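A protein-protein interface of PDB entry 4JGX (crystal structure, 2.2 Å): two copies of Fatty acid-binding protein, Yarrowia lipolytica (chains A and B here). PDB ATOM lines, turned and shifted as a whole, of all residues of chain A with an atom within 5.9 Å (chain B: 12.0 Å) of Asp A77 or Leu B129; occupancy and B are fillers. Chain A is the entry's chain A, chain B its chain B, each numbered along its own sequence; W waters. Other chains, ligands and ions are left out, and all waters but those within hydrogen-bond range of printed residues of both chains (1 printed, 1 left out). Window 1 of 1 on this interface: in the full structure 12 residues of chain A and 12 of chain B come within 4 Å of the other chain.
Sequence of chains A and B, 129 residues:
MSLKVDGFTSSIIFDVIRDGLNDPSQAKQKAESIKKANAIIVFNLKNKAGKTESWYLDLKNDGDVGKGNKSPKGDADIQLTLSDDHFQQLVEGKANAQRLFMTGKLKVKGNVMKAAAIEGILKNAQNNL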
ATOM      1  N   ASN A  38     -31.948  29.722   2.934  1.00  0.00           N
ATOM      2  CA  ASN A  38     -31.509  30.983   2.328  1.00  0.00           C
ATOM      3  C   ASN A  38     -30.635  30.778   1.069  1.00  0.00           C
ATOM      4  O   ASN A  38     -29.602  31.439   0.904  1.00  0.00           O
ATOM      5  CB  ASN A  38     -30.774  31.835   3.378  1.00  0.00           C
ATOM      6  CG  ASN A  38     -30.460  33.233   2.886  1.00  0.00           C
ATOM      7  OD1 ASN A  38     -31.292  33.885   2.247  1.00  0.00           O
ATOM      8  ND2 ASN A  38     -29.254  33.705   3.180  1.00  0.00           N
ATOM      9  N   ALA A  39     -31.054  29.860   0.191  1.00  0.00           N
ATOM     10  CA  ALA A  39     -30.200  29.377  -0.887  1.00  0.00           C
ATOM     11  C   ALA A  39     -31.003  28.985  -2.117  1.00  0.00           C
ATOM     12  O   ALA A  39     -32.089  28.422  -1.999  1.00  0.00           O
ATOM     13  CB  ALA A  39     -29.387  28.179  -0.413  1.00  0.00           C
ATOM     14  N   ILE A  40     -30.447  29.288  -3.289  1.00  0.00           N
ATOM     15  CA  ILE A  40     -30.949  28.784  -4.556  1.00  0.00           C
ATOM     16  C   ILE A  40     -30.093  27.573  -4.955  1.00  0.00           C
ATOM     17  O   ILE A  40     -28.862  27.673  -5.037  1.00  0.00           O
ATOM     18  CB  ILE A  40     -30.928  29.874  -5.650  1.00  0.00           C
ATOM     19  CG1 ILE A  40     -31.854  31.038  -5.249  1.00  0.00           C
ATOM     20  CG2 ILE A  40     -31.328  29.290  -7.000  1.00  0.00           C
ATOM     21  CD1 ILE A  40     -31.875  32.208  -6.208  1.00  0.00           C
ATOM     22  N   ILE A  41     -30.751  26.431  -5.154  1.00  0.00           N
ATOM     23  CA  ILE A  41     -30.092  25.166  -5.474  1.00  0.00           C
ATOM     24  C   ILE A  41     -30.442  24.778  -6.903  1.00  0.00           C
ATOM     25  O   ILE A  41     -31.609  24.690  -7.248  1.00  0.00           O
ATOM     26  CB  ILE A  41     -30.545  24.042  -4.519  1.00  0.00           C
ATOM     27  CG1 ILE A  41     -30.364  24.487  -3.067  1.00  0.00           C
ATOM     28  CG2 ILE A  41     -29.822  22.716  -4.813  1.00  0.00           C
ATOM     29  CD1 ILE A  41     -31.366  23.873  -2.119  1.00  0.00           C
ATOM     30  N   LYS A  60     -34.486  30.800  -1.133  1.00  0.00           N
ATOM     31  CA  LYS A  60     -33.962  32.078  -0.658  1.00  0.00           C
ATOM     32  C   LYS A  60     -35.041  33.154  -0.743  1.00  0.00           C
ATOM     33  O   LYS A  60     -35.253  33.892   0.208  1.00  0.00           O
ATOM     34  CB  LYS A  60     -32.708  32.484  -1.440  1.00  0.00           C
ATOM     35  CG  LYS A  60     -32.170  33.864  -1.074  1.00  0.00           C
ATOM     36  CD  LYS A  60     -30.710  34.039  -1.446  1.00  0.00           C
ATOM     37  CE  LYS A  60     -30.524  34.196  -2.944  1.00  0.00           C
ATOM     38  NZ  LYS A  60     -29.183  33.689  -3.356  1.00  0.00           N
ATOM     39  N   ASP A  75     -29.085  34.266  -8.949  1.00  0.00           N
ATOM     40  CA  ASP A  75     -28.155  33.187  -9.305  1.00  0.00           C
ATOM     41  C   ASP A  75     -28.187  32.035  -8.308  1.00  0.00           C
ATOM     42  O   ASP A  75     -28.708  32.169  -7.202  1.00  0.00           O
ATOM     43  CB  ASP A  75     -26.726  33.727  -9.396  1.00  0.00           C
ATOM     44  CG  ASP A  75     -26.602  34.891 -10.357  1.00  0.00           C
ATOM     45  OD1 ASP A  75     -27.307  34.887 -11.389  1.00  0.00           O
ATOM     46  OD2 ASP A  75     -25.802  35.807 -10.076  1.00  0.00           O
ATOM     47  N   ALA A  76     -27.614  30.905  -8.694  1.00  0.00           N
ATOM     48  CA  ALA A  76     -27.594  29.741  -7.814  1.00  0.00           C
ATOM     49  C   ALA A  76     -26.531  29.898  -6.729  1.00  0.00           C
ATOM     50  O   ALA A  76     -25.442  30.403  -6.994  1.00  0.00           O
ATOM     51  CB  ALA A  76     -27.339  28.482  -8.622  1.00  0.00           C
ATOM     52  N   ASP A  77     -26.844  29.458  -5.517  1.00  0.00           N
ATOM     53  CA  ASP A  77     -25.844  29.385  -4.448  1.00  0.00           C
ATOM     54  C   ASP A  77     -25.070  28.076  -4.446  1.00  0.00           C
ATOM     55  O   ASP A  77     -23.932  28.012  -3.996  1.00  0.00           O
ATOM     56  CB  ASP A  77     -26.524  29.550  -3.105  1.00  0.00           C
ATOM     57  CG  ASP A  77     -27.065  30.927  -2.922  1.00  0.00           C
ATOM     58  OD1 ASP A  77     -26.246  31.868  -2.817  1.00  0.00           O
ATOM     59  OD2 ASP A  77     -28.295  31.067  -2.902  1.00  0.00           O
ATOM     60  N   ILE A  78     -25.706  27.028  -4.944  1.00  0.00           N
ATOM     61  CA  ILE A  78     -25.139  25.704  -4.877  1.00  0.00           C
ATOM     62  C   ILE A  78     -25.662  24.903  -6.054  1.00  0.00           C
ATOM     63  O   ILE A  78     -26.794  25.103  -6.517  1.00  0.00           O
ATOM     64  CB  ILE A  78     -25.400  25.050  -3.496  1.00  0.00           C
ATOM     65  CG1 ILE A  78     -24.961  23.592  -3.465  1.00  0.00           C
ATOM     66  CG2 ILE A  78     -26.840  25.190  -3.051  1.00  0.00           C
ATOM     67  CD1 ILE A  78     -23.576  23.441  -2.875  1.00  0.00           C
ATOM     68  N   GLN A  79     -24.820  24.022  -6.566  1.00  0.00           N
ATOM     69  CA  GLN A  79     -25.189  23.226  -7.721  1.00  0.00           C
ATOM     70  C   GLN A  79     -24.851  21.746  -7.533  1.00  0.00           C
ATOM     71  O   GLN A  79     -23.725  21.394  -7.178  1.00  0.00           O
ATOM     72  CB  GLN A  79     -24.521  23.804  -8.958  1.00  0.00           C
ATOM     73  CG  GLN A  79     -24.617  22.943 -10.180  1.00  0.00           C
ATOM     74  CD  GLN A  79     -23.972  23.619 -11.369  1.00  0.00           C
ATOM     75  OE1 GLN A  79     -22.881  23.242 -11.788  1.00  0.00           O
ATOM     76  NE2 GLN A  79     -24.633  24.639 -11.903  1.00  0.00           N
ATOM     77  N   LYS A 109     -20.886  22.028  -6.357  1.00  0.00           N
ATOM     78  CA  LYS A 109     -20.189  23.277  -6.618  1.00  0.00           C
ATOM     79  C   LYS A 109     -20.912  24.362  -5.848  1.00  0.00           C
ATOM     80  O   LYS A 109     -22.132  24.304  -5.698  1.00  0.00           O
ATOM     81  CB  LYS A 109     -20.303  23.655  -8.086  1.00  0.00           C
ATOM     82  CG  LYS A 109     -19.250  23.098  -9.004  1.00  0.00           C
ATOM     83  CD  LYS A 109     -19.287  23.894 -10.297  1.00  0.00           C
ATOM     84  CE  LYS A 109     -18.403  23.258 -11.359  1.00  0.00           C
ATOM     85  NZ  LYS A 109     -18.345  24.119 -12.569  1.00  0.00           N
ATOM     86  N   GLY A 110     -20.162  25.363  -5.388  1.00  0.00           N
ATOM     87  CA  GLY A 110     -20.770  26.530  -4.812  1.00  0.00           C
ATOM     88  C   GLY A 110     -20.425  26.685  -3.355  1.00  0.00           C
ATOM     89  O   GLY A 110     -19.378  26.209  -2.877  1.00  0.00           O
ATOM     90  N   ASN A 111     -21.329  27.348  -2.652  1.00  0.00           N
ATOM     91  CA  ASN A 111     -21.099  27.799  -1.297  1.00  0.00           C
ATOM     92  C   ASN A 111     -21.165  26.651  -0.283  1.00  0.00           C
ATOM     93  O   ASN A 111     -22.235  26.076  -0.066  1.00  0.00           O
ATOM     94  CB  ASN A 111     -22.136  28.880  -0.967  1.00  0.00           C
ATOM     95  CG  ASN A 111     -21.819  29.635   0.308  1.00  0.00           C
ATOM     96  OD1 ASN A 111     -20.907  29.284   1.053  1.00  0.00           O
ATOM     97  ND2 ASN A 111     -22.573  30.696   0.556  1.00  0.00           N
ATOM     98  N   LYS A 114     -23.865  26.890   2.393  1.00  0.00           N
ATOM     99  CA  LYS A 114     -25.194  26.545   1.893  1.00  0.00           C
ATOM    100  C   LYS A 114     -25.314  25.047   1.724  1.00  0.00           C
ATOM    101  O   LYS A 114     -26.327  24.472   2.090  1.00  0.00           O
ATOM    102  CB  LYS A 114     -25.491  27.237   0.563  1.00  0.00           C
ATOM    103  CG  LYS A 114     -25.357  28.751   0.595  1.00  0.00           C
ATOM    104  CD  LYS A 114     -26.423  29.417   1.432  1.00  0.00           C
ATOM    105  CE  LYS A 114     -26.444  30.904   1.152  1.00  0.00           C
ATOM    106  NZ  LYS A 114     -27.153  31.611   2.248  1.00  0.00           N
ATOM    107  N   VAL B  16     -15.407  18.965   0.409  1.00  0.00           N
ATOM    108  CA  VAL B  16     -16.108  19.964  -0.369  1.00  0.00           C
ATOM    109  C   VAL B  16     -15.278  21.245  -0.457  1.00  0.00           C
ATOM    110  O   VAL B  16     -15.267  21.887  -1.503  1.00  0.00           O
ATOM    111  CB  VAL B  16     -17.510  20.248   0.193  1.00  0.00           C
ATOM    112  CG1 VAL B  16     -18.148  21.446  -0.501  1.00  0.00           C
ATOM    113  CG2 VAL B  16     -18.382  19.012   0.026  1.00  0.00           C
ATOM    114  N   ILE B  17     -14.577  21.591   0.630  1.00  0.00           N
ATOM    115  CA  ILE B  17     -13.720  22.764   0.660  1.00  0.00           C
ATOM    116  C   ILE B  17     -12.517  22.570  -0.263  1.00  0.00           C
ATOM    117  O   ILE B  17     -12.133  23.486  -1.010  1.00  0.00           O
ATOM    118  CB  ILE B  17     -13.243  23.098   2.102  1.00  0.00           C
ATOM    119  CG1 ILE B  17     -14.378  23.741   2.936  1.00  0.00           C
ATOM    120  CG2 ILE B  17     -12.028  24.023   2.068  1.00  0.00           C
ATOM    121  CD1 ILE B  17     -14.096  23.747   4.439  1.00  0.00           C
ATOM    122  N   ARG B  18     -11.909  21.385  -0.210  1.00  0.00           N
ATOM    123  CA  ARG B  18     -10.774  21.086  -1.087  1.00  0.00           C
ATOM    124  C   ARG B  18     -11.144  21.185  -2.570  1.00  0.00           C
ATOM    125  O   ARG B  18     -10.441  21.826  -3.351  1.00  0.00           O
ATOM    126  CB  ARG B  18     -10.179  19.694  -0.791  1.00  0.00           C
ATOM    127  CG  ARG B  18      -8.969  19.385  -1.694  1.00  0.00           C
ATOM    128  CD  ARG B  18      -8.184  18.159  -1.256  1.00  0.00           C
ATOM    129  NE  ARG B  18      -8.992  16.949  -1.295  1.00  0.00           N
ATOM    130  CZ  ARG B  18      -8.559  15.740  -0.955  1.00  0.00           C
ATOM    131  NH1 ARG B  18      -7.324  15.552  -0.506  1.00  0.00           N
ATOM    132  NH2 ARG B  18      -9.386  14.712  -1.041  1.00  0.00           N
ATOM    133  N   ASP B  19     -12.239  20.527  -2.956  1.00  0.00           N
ATOM    134  CA  ASP B  19     -12.734  20.602  -4.349  1.00  0.00           C
ATOM    135  C   ASP B  19     -12.980  22.037  -4.800  1.00  0.00           C
ATOM    136  O   ASP B  19     -12.655  22.381  -5.931  1.00  0.00           O
ATOM    137  CB  ASP B  19     -14.017  19.800  -4.549  1.00  0.00           C
ATOM    138  CG  ASP B  19     -13.782  18.305  -4.498  1.00  0.00           C
ATOM    139  OD1 ASP B  19     -12.675  17.848  -4.852  1.00  0.00           O
ATOM    140  OD2 ASP B  19     -14.707  17.570  -4.104  1.00  0.00           O
ATOM    141  N   GLY B  20     -13.566  22.860  -3.921  1.00  0.00           N
ATOM    142  CA  GLY B  20     -13.870  24.247  -4.246  1.00  0.00           C
ATOM    143  C   GLY B  20     -12.606  25.078  -4.431  1.00  0.00           C
ATOM    144  O   GLY B  20     -12.466  25.796  -5.416  1.00  0.00           O
ATOM    145  N   LEU B  21     -11.691  24.970  -3.481  1.00  0.00           N
ATOM    146  CA  LEU B  21     -10.436  25.720  -3.488  1.00  0.00           C
ATOM    147  C   LEU B  21      -9.476  25.301  -4.598  1.00  0.00           C
ATOM    148  O   LEU B  21      -8.782  26.157  -5.150  1.00  0.00           O
ATOM    149  CB  LEU B  21      -9.727  25.580  -2.131  1.00  0.00           C
ATOM    150  CG  LEU B  21      -8.387  26.307  -2.011  1.00  0.00           C
ATOM    151  CD1 LEU B  21      -8.620  27.789  -1.725  1.00  0.00           C
ATOM    152  CD2 LEU B  21      -7.529  25.677  -0.925  1.00  0.00           C
ATOM    153  N   ASN B  22      -9.433  23.996  -4.904  1.00  0.00           N
ATOM    154  CA  ASN B  22      -8.497  23.444  -5.882  1.00  0.00           C
ATOM    155  C   ASN B  22      -9.012  23.501  -7.325  1.00  0.00           C
ATOM    156  O   ASN B  22      -8.244  23.311  -8.278  1.00  0.00           O
ATOM    157  CB  ASN B  22      -8.109  21.995  -5.518  1.00  0.00           C
ATOM    158  CG  ASN B  22      -7.124  21.917  -4.363  1.00  0.00           C
ATOM    159  OD1 ASN B  22      -6.614  22.937  -3.887  1.00  0.00           O
ATOM    160  ND2 ASN B  22      -6.840  20.700  -3.911  1.00  0.00           N
ATOM    161  N   ASP B  23     -10.317  23.717  -7.485  1.00  0.00           N
ATOM    162  CA  ASP B  23     -10.904  23.910  -8.806  1.00  0.00           C
ATOM    163  C   ASP B  23     -10.019  24.878  -9.611  1.00  0.00           C
ATOM    164  O   ASP B  23      -9.792  26.009  -9.165  1.00  0.00           O
ATOM    165  CB  ASP B  23     -12.326  24.479  -8.677  1.00  0.00           C
ATOM    166  CG  ASP B  23     -13.074  24.479  -9.999  1.00  0.00           C
ATOM    167  OD1 ASP B  23     -12.412  24.452 -11.050  1.00  0.00           O
ATOM    168  OD2 ASP B  23     -14.320  24.478  -9.988  1.00  0.00           O
ATOM    169  N   PRO B  24      -9.496  24.431 -10.785  1.00  0.00           N
ATOM    170  CA  PRO B  24      -8.589  25.312 -11.506  1.00  0.00           C
ATOM    171  C   PRO B  24      -9.254  26.620 -11.951  1.00  0.00           C
ATOM    172  O   PRO B  24      -8.560  27.624 -12.133  1.00  0.00           O
ATOM    173  CB  PRO B  24      -8.119  24.468 -12.708  1.00  0.00           C
ATOM    174  CG  PRO B  24      -9.052  23.322 -12.792  1.00  0.00           C
ATOM    175  CD  PRO B  24      -9.599  23.100 -11.413  1.00  0.00           C
ATOM    176  N   SER B  25     -10.584  26.621 -12.084  1.00  0.00           N
ATOM    177  CA  SER B  25     -11.339  27.872 -12.321  1.00  0.00           C
ATOM    178  C   SER B  25     -11.297  28.853 -11.150  1.00  0.00           C
ATOM    179  O   SER B  25     -11.717  29.996 -11.287  1.00  0.00           O
ATOM    180  CB  SER B  25     -12.790  27.575 -12.654  1.00  0.00           C
ATOM    181  OG  SER B  25     -12.858  26.967 -13.920  1.00  0.00           O
ATOM    182  N   GLN B  26     -10.811  28.407 -10.004  1.00  0.00           N
ATOM    183  CA  GLN B  26     -10.693  29.274  -8.837  1.00  0.00           C
ATOM    184  C   GLN B  26      -9.286  29.834  -8.680  1.00  0.00           C
ATOM    185  O   GLN B  26      -8.957  30.408  -7.645  1.00  0.00           O
ATOM    186  CB  GLN B  26     -11.098  28.514  -7.573  1.00  0.00           C
ATOM    187  CG  GLN B  26     -12.599  28.346  -7.440  1.00  0.00           C
ATOM    188  CD  GLN B  26     -13.316  29.678  -7.294  1.00  0.00           C
ATOM    189  OE1 GLN B  26     -13.904  30.174  -8.259  1.00  0.00           O
ATOM    190  NE2 GLN B  26     -13.250  30.279  -6.097  1.00  0.00           N
ATOM    191  N   ALA B  27      -8.460  29.675  -9.711  1.00  0.00           N
ATOM    192  CA  ALA B  27      -7.055  30.085  -9.644  1.00  0.00           C
ATOM    193  C   ALA B  27      -6.848  31.504  -9.098  1.00  0.00           C
ATOM    194  O   ALA B  27      -5.990  31.717  -8.244  1.00  0.00           O
ATOM    195  CB  ALA B  27      -6.385  29.934 -11.010  1.00  0.00           C
ATOM    196  N   LYS B  28      -7.629  32.463  -9.596  1.00  0.00           N
ATOM    197  CA  LYS B  28      -7.498  33.862  -9.192  1.00  0.00           C
ATOM    198  C   LYS B  28      -7.873  34.054  -7.727  1.00  0.00           C
ATOM    199  O   LYS B  28      -7.114  34.656  -6.950  1.00  0.00           O
ATOM    200  CB  LYS B  28      -8.341  34.769 -10.097  1.00  0.00           C
ATOM    201  CG  LYS B  28      -8.359  36.223  -9.665  1.00  0.00           C
ATOM    202  CD  LYS B  28      -8.543  37.180 -10.827  1.00  0.00           C
ATOM    203  CE  LYS B  28      -8.745  38.594 -10.294  1.00  0.00           C
ATOM    204  NZ  LYS B  28      -8.839  39.602 -11.378  1.00  0.00           N
ATOM    205  N   GLN B  29      -9.037  33.509  -7.369  1.00  0.00           N
ATOM    206  CA  GLN B  29      -9.594  33.583  -6.024  1.00  0.00           C
ATOM    207  C   GLN B  29      -8.643  32.906  -5.045  1.00  0.00           C
ATOM    208  O   GLN B  29      -8.379  33.432  -3.963  1.00  0.00           O
ATOM    209  CB  GLN B  29     -10.969  32.893  -5.972  1.00  0.00           C
ATOM    210  CG  GLN B  29     -12.081  33.545  -6.796  1.00  0.00           C
ATOM    211  CD  GLN B  29     -11.944  33.395  -8.317  1.00  0.00           C
ATOM    212  OE1 GLN B  29     -11.198  32.555  -8.839  1.00  0.00           O
ATOM    213  NE2 GLN B  29     -12.680  34.228  -9.040  1.00  0.00           N
ATOM    214  N   LYS B  30      -8.120  31.743  -5.437  1.00  0.00           N
ATOM    215  CA  LYS B  30      -7.182  31.013  -4.606  1.00  0.00           C
ATOM    216  C   LYS B  30      -5.976  31.896  -4.288  1.00  0.00           C
ATOM    217  O   LYS B  30      -5.611  32.054  -3.114  1.00  0.00           O
ATOM    218  CB  LYS B  30      -6.751  29.718  -5.307  1.00  0.00           C
ATOM    219  CG  LYS B  30      -5.876  28.820  -4.441  1.00  0.00           C
ATOM    220  CD  LYS B  30      -5.641  27.449  -5.049  1.00  0.00           C
ATOM    221  CE  LYS B  30      -4.626  27.513  -6.183  1.00  0.00           C
ATOM    222  NZ  LYS B  30      -4.884  26.414  -7.161  1.00  0.00           N
ATOM    223  N   VAL B  91     -20.116  25.727  10.245  1.00  0.00           N
ATOM    224  CA  VAL B  91     -20.086  25.729   8.779  1.00  0.00           C
ATOM    225  C   VAL B  91     -21.499  26.018   8.242  1.00  0.00           C
ATOM    226  O   VAL B  91     -21.664  26.763   7.275  1.00  0.00           O
ATOM    227  CB  VAL B  91     -19.462  24.430   8.195  1.00  0.00           C
ATOM    228  CG1 VAL B  91     -19.469  24.464   6.667  1.00  0.00           C
ATOM    229  CG2 VAL B  91     -18.034  24.266   8.693  1.00  0.00           C
ATOM    230  N   GLU B  92     -22.506  25.465   8.916  1.00  0.00           N
ATOM    231  CA  GLU B  92     -23.903  25.753   8.605  1.00  0.00           C
ATOM    232  C   GLU B  92     -24.351  27.206   8.834  1.00  0.00           C
ATOM    233  O   GLU B  92     -25.300  27.663   8.200  1.00  0.00           O
ATOM    234  CB  GLU B  92     -24.797  24.863   9.443  1.00  0.00           C
ATOM    235  CG  GLU B  92     -24.771  23.415   9.029  1.00  0.00           C
ATOM    236  CD  GLU B  92     -25.888  22.654   9.694  1.00  0.00           C
ATOM    237  OE1 GLU B  92     -27.006  23.213   9.777  1.00  0.00           O
ATOM    238  OE2 GLU B  92     -25.647  21.514  10.141  1.00  0.00           O
ATOM    239  N   LEU B 122     -11.836  32.352   3.415  1.00  0.00           N
ATOM    240  CA  LEU B 122     -12.081  30.989   2.955  1.00  0.00           C
ATOM    241  C   LEU B 122     -13.306  30.932   2.044  1.00  0.00           C
ATOM    242  O   LEU B 122     -13.210  30.469   0.894  1.00  0.00           O
ATOM    243  CB  LEU B 122     -12.237  30.023   4.132  1.00  0.00           C
ATOM    244  CG  LEU B 122     -12.434  28.541   3.754  1.00  0.00           C
ATOM    245  CD1 LEU B 122     -11.390  28.031   2.766  1.00  0.00           C
ATOM    246  CD2 LEU B 122     -12.510  27.657   4.998  1.00  0.00           C
ATOM    247  N   LYS B 123     -14.436  31.424   2.563  1.00  0.00           N
ATOM    248  CA  LYS B 123     -15.666  31.573   1.788  1.00  0.00           C
ATOM    249  C   LYS B 123     -15.424  32.016   0.346  1.00  0.00           C
ATOM    250  O   LYS B 123     -15.939  31.394  -0.583  1.00  0.00           O
ATOM    251  CB  LYS B 123     -16.637  32.525   2.489  1.00  0.00           C
ATOM    252  CG  LYS B 123     -17.636  31.823   3.390  1.00  0.00           C
ATOM    253  CD  LYS B 123     -18.630  32.815   3.977  1.00  0.00           C
ATOM    254  CE  LYS B 123     -19.843  32.112   4.565  1.00  0.00           C
ATOM    255  NZ  LYS B 123     -20.392  32.879   5.719  1.00  0.00           N
ATOM    256  N   ASN B 124     -14.633  33.073   0.161  1.00  0.00           N
ATOM    257  CA  ASN B 124     -14.349  33.596  -1.176  1.00  0.00           C
ATOM    258  C   ASN B 124     -13.546  32.643  -2.076  1.00  0.00           C
ATOM    259  O   ASN B 124     -13.832  32.513  -3.274  1.00  0.00           O
ATOM    260  CB  ASN B 124     -13.626  34.945  -1.092  1.00  0.00           C
ATOM    261  CG  ASN B 124     -13.262  35.494  -2.467  1.00  0.00           C
ATOM    262  OD1 ASN B 124     -14.142  35.823  -3.262  1.00  0.00           O
ATOM    263  ND2 ASN B 124     -11.960  35.577  -2.760  1.00  0.00           N
ATOM    264  N   ALA B 125     -12.535  31.997  -1.506  1.00  0.00           N
ATOM    265  CA  ALA B 125     -11.647  31.119  -2.280  1.00  0.00           C
ATOM    266  C   ALA B 125     -12.303  29.789  -2.690  1.00  0.00           C
ATOM    267  O   ALA B 125     -12.129  29.315  -3.829  1.00  0.00           O
ATOM    268  CB  ALA B 125     -10.369  30.850  -1.503  1.00  0.00           C
ATOM    269  N   GLN B 126     -13.037  29.204  -1.741  1.00  0.00           N
ATOM    270  CA  GLN B 126     -13.727  27.928  -1.911  1.00  0.00           C
ATOM    271  C   GLN B 126     -14.962  28.012  -2.840  1.00  0.00           C
ATOM    272  O   GLN B 126     -15.325  27.025  -3.489  1.00  0.00           O
ATOM    273  CB  GLN B 126     -14.117  27.369  -0.528  1.00  0.00           C
ATOM    274  CG  GLN B 126     -14.763  25.984  -0.529  1.00  0.00           C
ATOM    275  CD  GLN B 126     -16.242  26.006  -0.911  1.00  0.00           C
ATOM    276  OE1 GLN B 126     -16.996  26.886  -0.462  1.00  0.00           O
ATOM    277  NE2 GLN B 126     -16.662  25.050  -1.761  1.00  0.00           N
ATOM    278  N   ASN B 127     -15.600  29.178  -2.903  1.00  0.00           N
ATOM    279  CA  ASN B 127     -16.869  29.297  -3.597  1.00  0.00           C
ATOM    280  C   ASN B 127     -16.745  29.275  -5.117  1.00  0.00           C
ATOM    281  O   ASN B 127     -16.727  30.317  -5.764  1.00  0.00           O
ATOM    282  CB  ASN B 127     -17.631  30.527  -3.114  1.00  0.00           C
ATOM    283  CG  ASN B 127     -19.099  30.482  -3.490  1.00  0.00           C
ATOM    284  OD1 ASN B 127     -19.485  29.869  -4.491  1.00  0.00           O
ATOM    285  ND2 ASN B 127     -19.929  31.135  -2.689  1.00  0.00           N
ATOM    286  N   ASN B 128     -16.708  28.068  -5.674  1.00  0.00           N
ATOM    287  CA  ASN B 128     -16.417  27.856  -7.095  1.00  0.00           C
ATOM    288  C   ASN B 128     -17.613  27.803  -8.051  1.00  0.00           C
ATOM    289  O   ASN B 128     -17.506  27.193  -9.118  1.00  0.00           O
ATOM    290  CB  ASN B 128     -15.576  26.584  -7.287  1.00  0.00           C
ATOM    291  CG  ASN B 128     -16.315  25.309  -6.879  1.00  0.00           C
ATOM    292  OD1 ASN B 128     -17.177  25.306  -5.975  1.00  0.00           O
ATOM    293  ND2 ASN B 128     -15.958  24.209  -7.531  1.00  0.00           N
ATOM    294  N   LEU B 129     -18.735  28.426  -7.693  1.00  0.00           N
ATOM    295  CA  LEU B 129     -19.890  28.443  -8.608  1.00  0.00           C
ATOM    296  C   LEU B 129     -19.845  29.633  -9.568  1.00  0.00           C
ATOM    297  O   LEU B 129     -19.912  30.787  -9.131  1.00  0.00           O
ATOM    298  CB  LEU B 129     -21.227  28.391  -7.842  1.00  0.00           C
ATOM    299  CG  LEU B 129     -22.515  28.131  -8.639  1.00  0.00           C
ATOM    300  CD1 LEU B 129     -22.323  27.064  -9.708  1.00  0.00           C
ATOM    301  CD2 LEU B 129     -23.650  27.745  -7.703  1.00  0.00           C
HETATM  302  O   HOH W   1     -15.978  25.544 -11.618  1.00  0.00           O
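Ala A39 touches none of the printed residues of chain B.
No residue of chain B comes within 4 Å of Ile A40.
No residue of chain B comes within 4 Å of Ile A41.
Ala A76 touches one residue of chain B.
Of the printed residues of chain B, Lys A109 touches Asn B128.
Gly A110 touches just these residues of chain B: Gln B126 (3.2 Å), Asn B127 (3.5 Å), Asn B128 (3.0 Å) and Leu B129 (3.6 Å).
No residue of chain B comes within 4 Å of Lys A114.
Printed residues of chain A within 4 Å of Asn B127: Gly A110 (3.5 Å) and Asn A111 (3.6 Å).
Printed residues of chain A within 4 Å of Asn B128: Lys A109 and Gly A110.
The nearest printed residue of chain A that does not touch Leu B129 is Gln A79 (4.003 Å).
NE2 of Gln B126 sits at hydrogen-bond distance from O of Gly A110.
OD1 of Asn B128 lies within hydrogen-bond range of N of Gly A110 (3.0 Å).
No position is printed for both chains.
Of the 9 pairs that touch across the chains among the printed residues, none has its exchanged pair printed and touching as well.
Of the 25 printed residues of chain B, 4 touch a printed residue of chain A.
Hydrophobic or aromatic side chains of chain B that line the printed part of chain A: Leu B129.
Among the printed residues, no Asp or Glu carboxylate lies within 4 Å of a Lys or Arg side-chain nitrogen of the other chain.
The side-chain amino group (NZ) of Lys A60 lies within salt-bridge range of the side-chain carboxylate (OD2) of Asp A77.
The backbone carbonyl oxygen of Asn B127 lies within hydrogen-bond range of the side-chain amide nitrogen of Gln B26, 3.5 Å away.
O of Ile A40 is in hydrogen-bond range of N of Asp A77.
The backbone carbonyl oxygen of Lys A109 is in hydrogen-bond range of the backbone NH of Gln A79.
The side-chain amide nitrogen of Gln B126 is in hydrogen-bond range of the backbone carbonyl oxygen of Val B16 (3.5 Å).
The backbone carbonyl oxygen (O) of Asp A77 is in hydrogen-bond range of the backbone NH (N) of Asn A111, at 3.0 Å.
Water W1 lies within hydrogen-bond range of OD2 of Asp B23 (2.6 Å), NZ of Lys A109 (2.9 Å) and O of Asn B128 (3.4 Å).
Ala A76 touches Leu B129 (O to CD2, 3.3 Å).
Leu B129 touches Asp A77 (CD2 to C, 3.6 Å).
Leu B129 touches Ile A78.
Asn B128 touches Lys A109 (OD1 to CA, 3.7 Å).
C of Gly A110 touches OD1 of Asn B127, 3.5 Å away.
Leu B129 touches Gly A110.
Asn A111 touches Asn B127 (CB to ND2, 3.6 Å).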
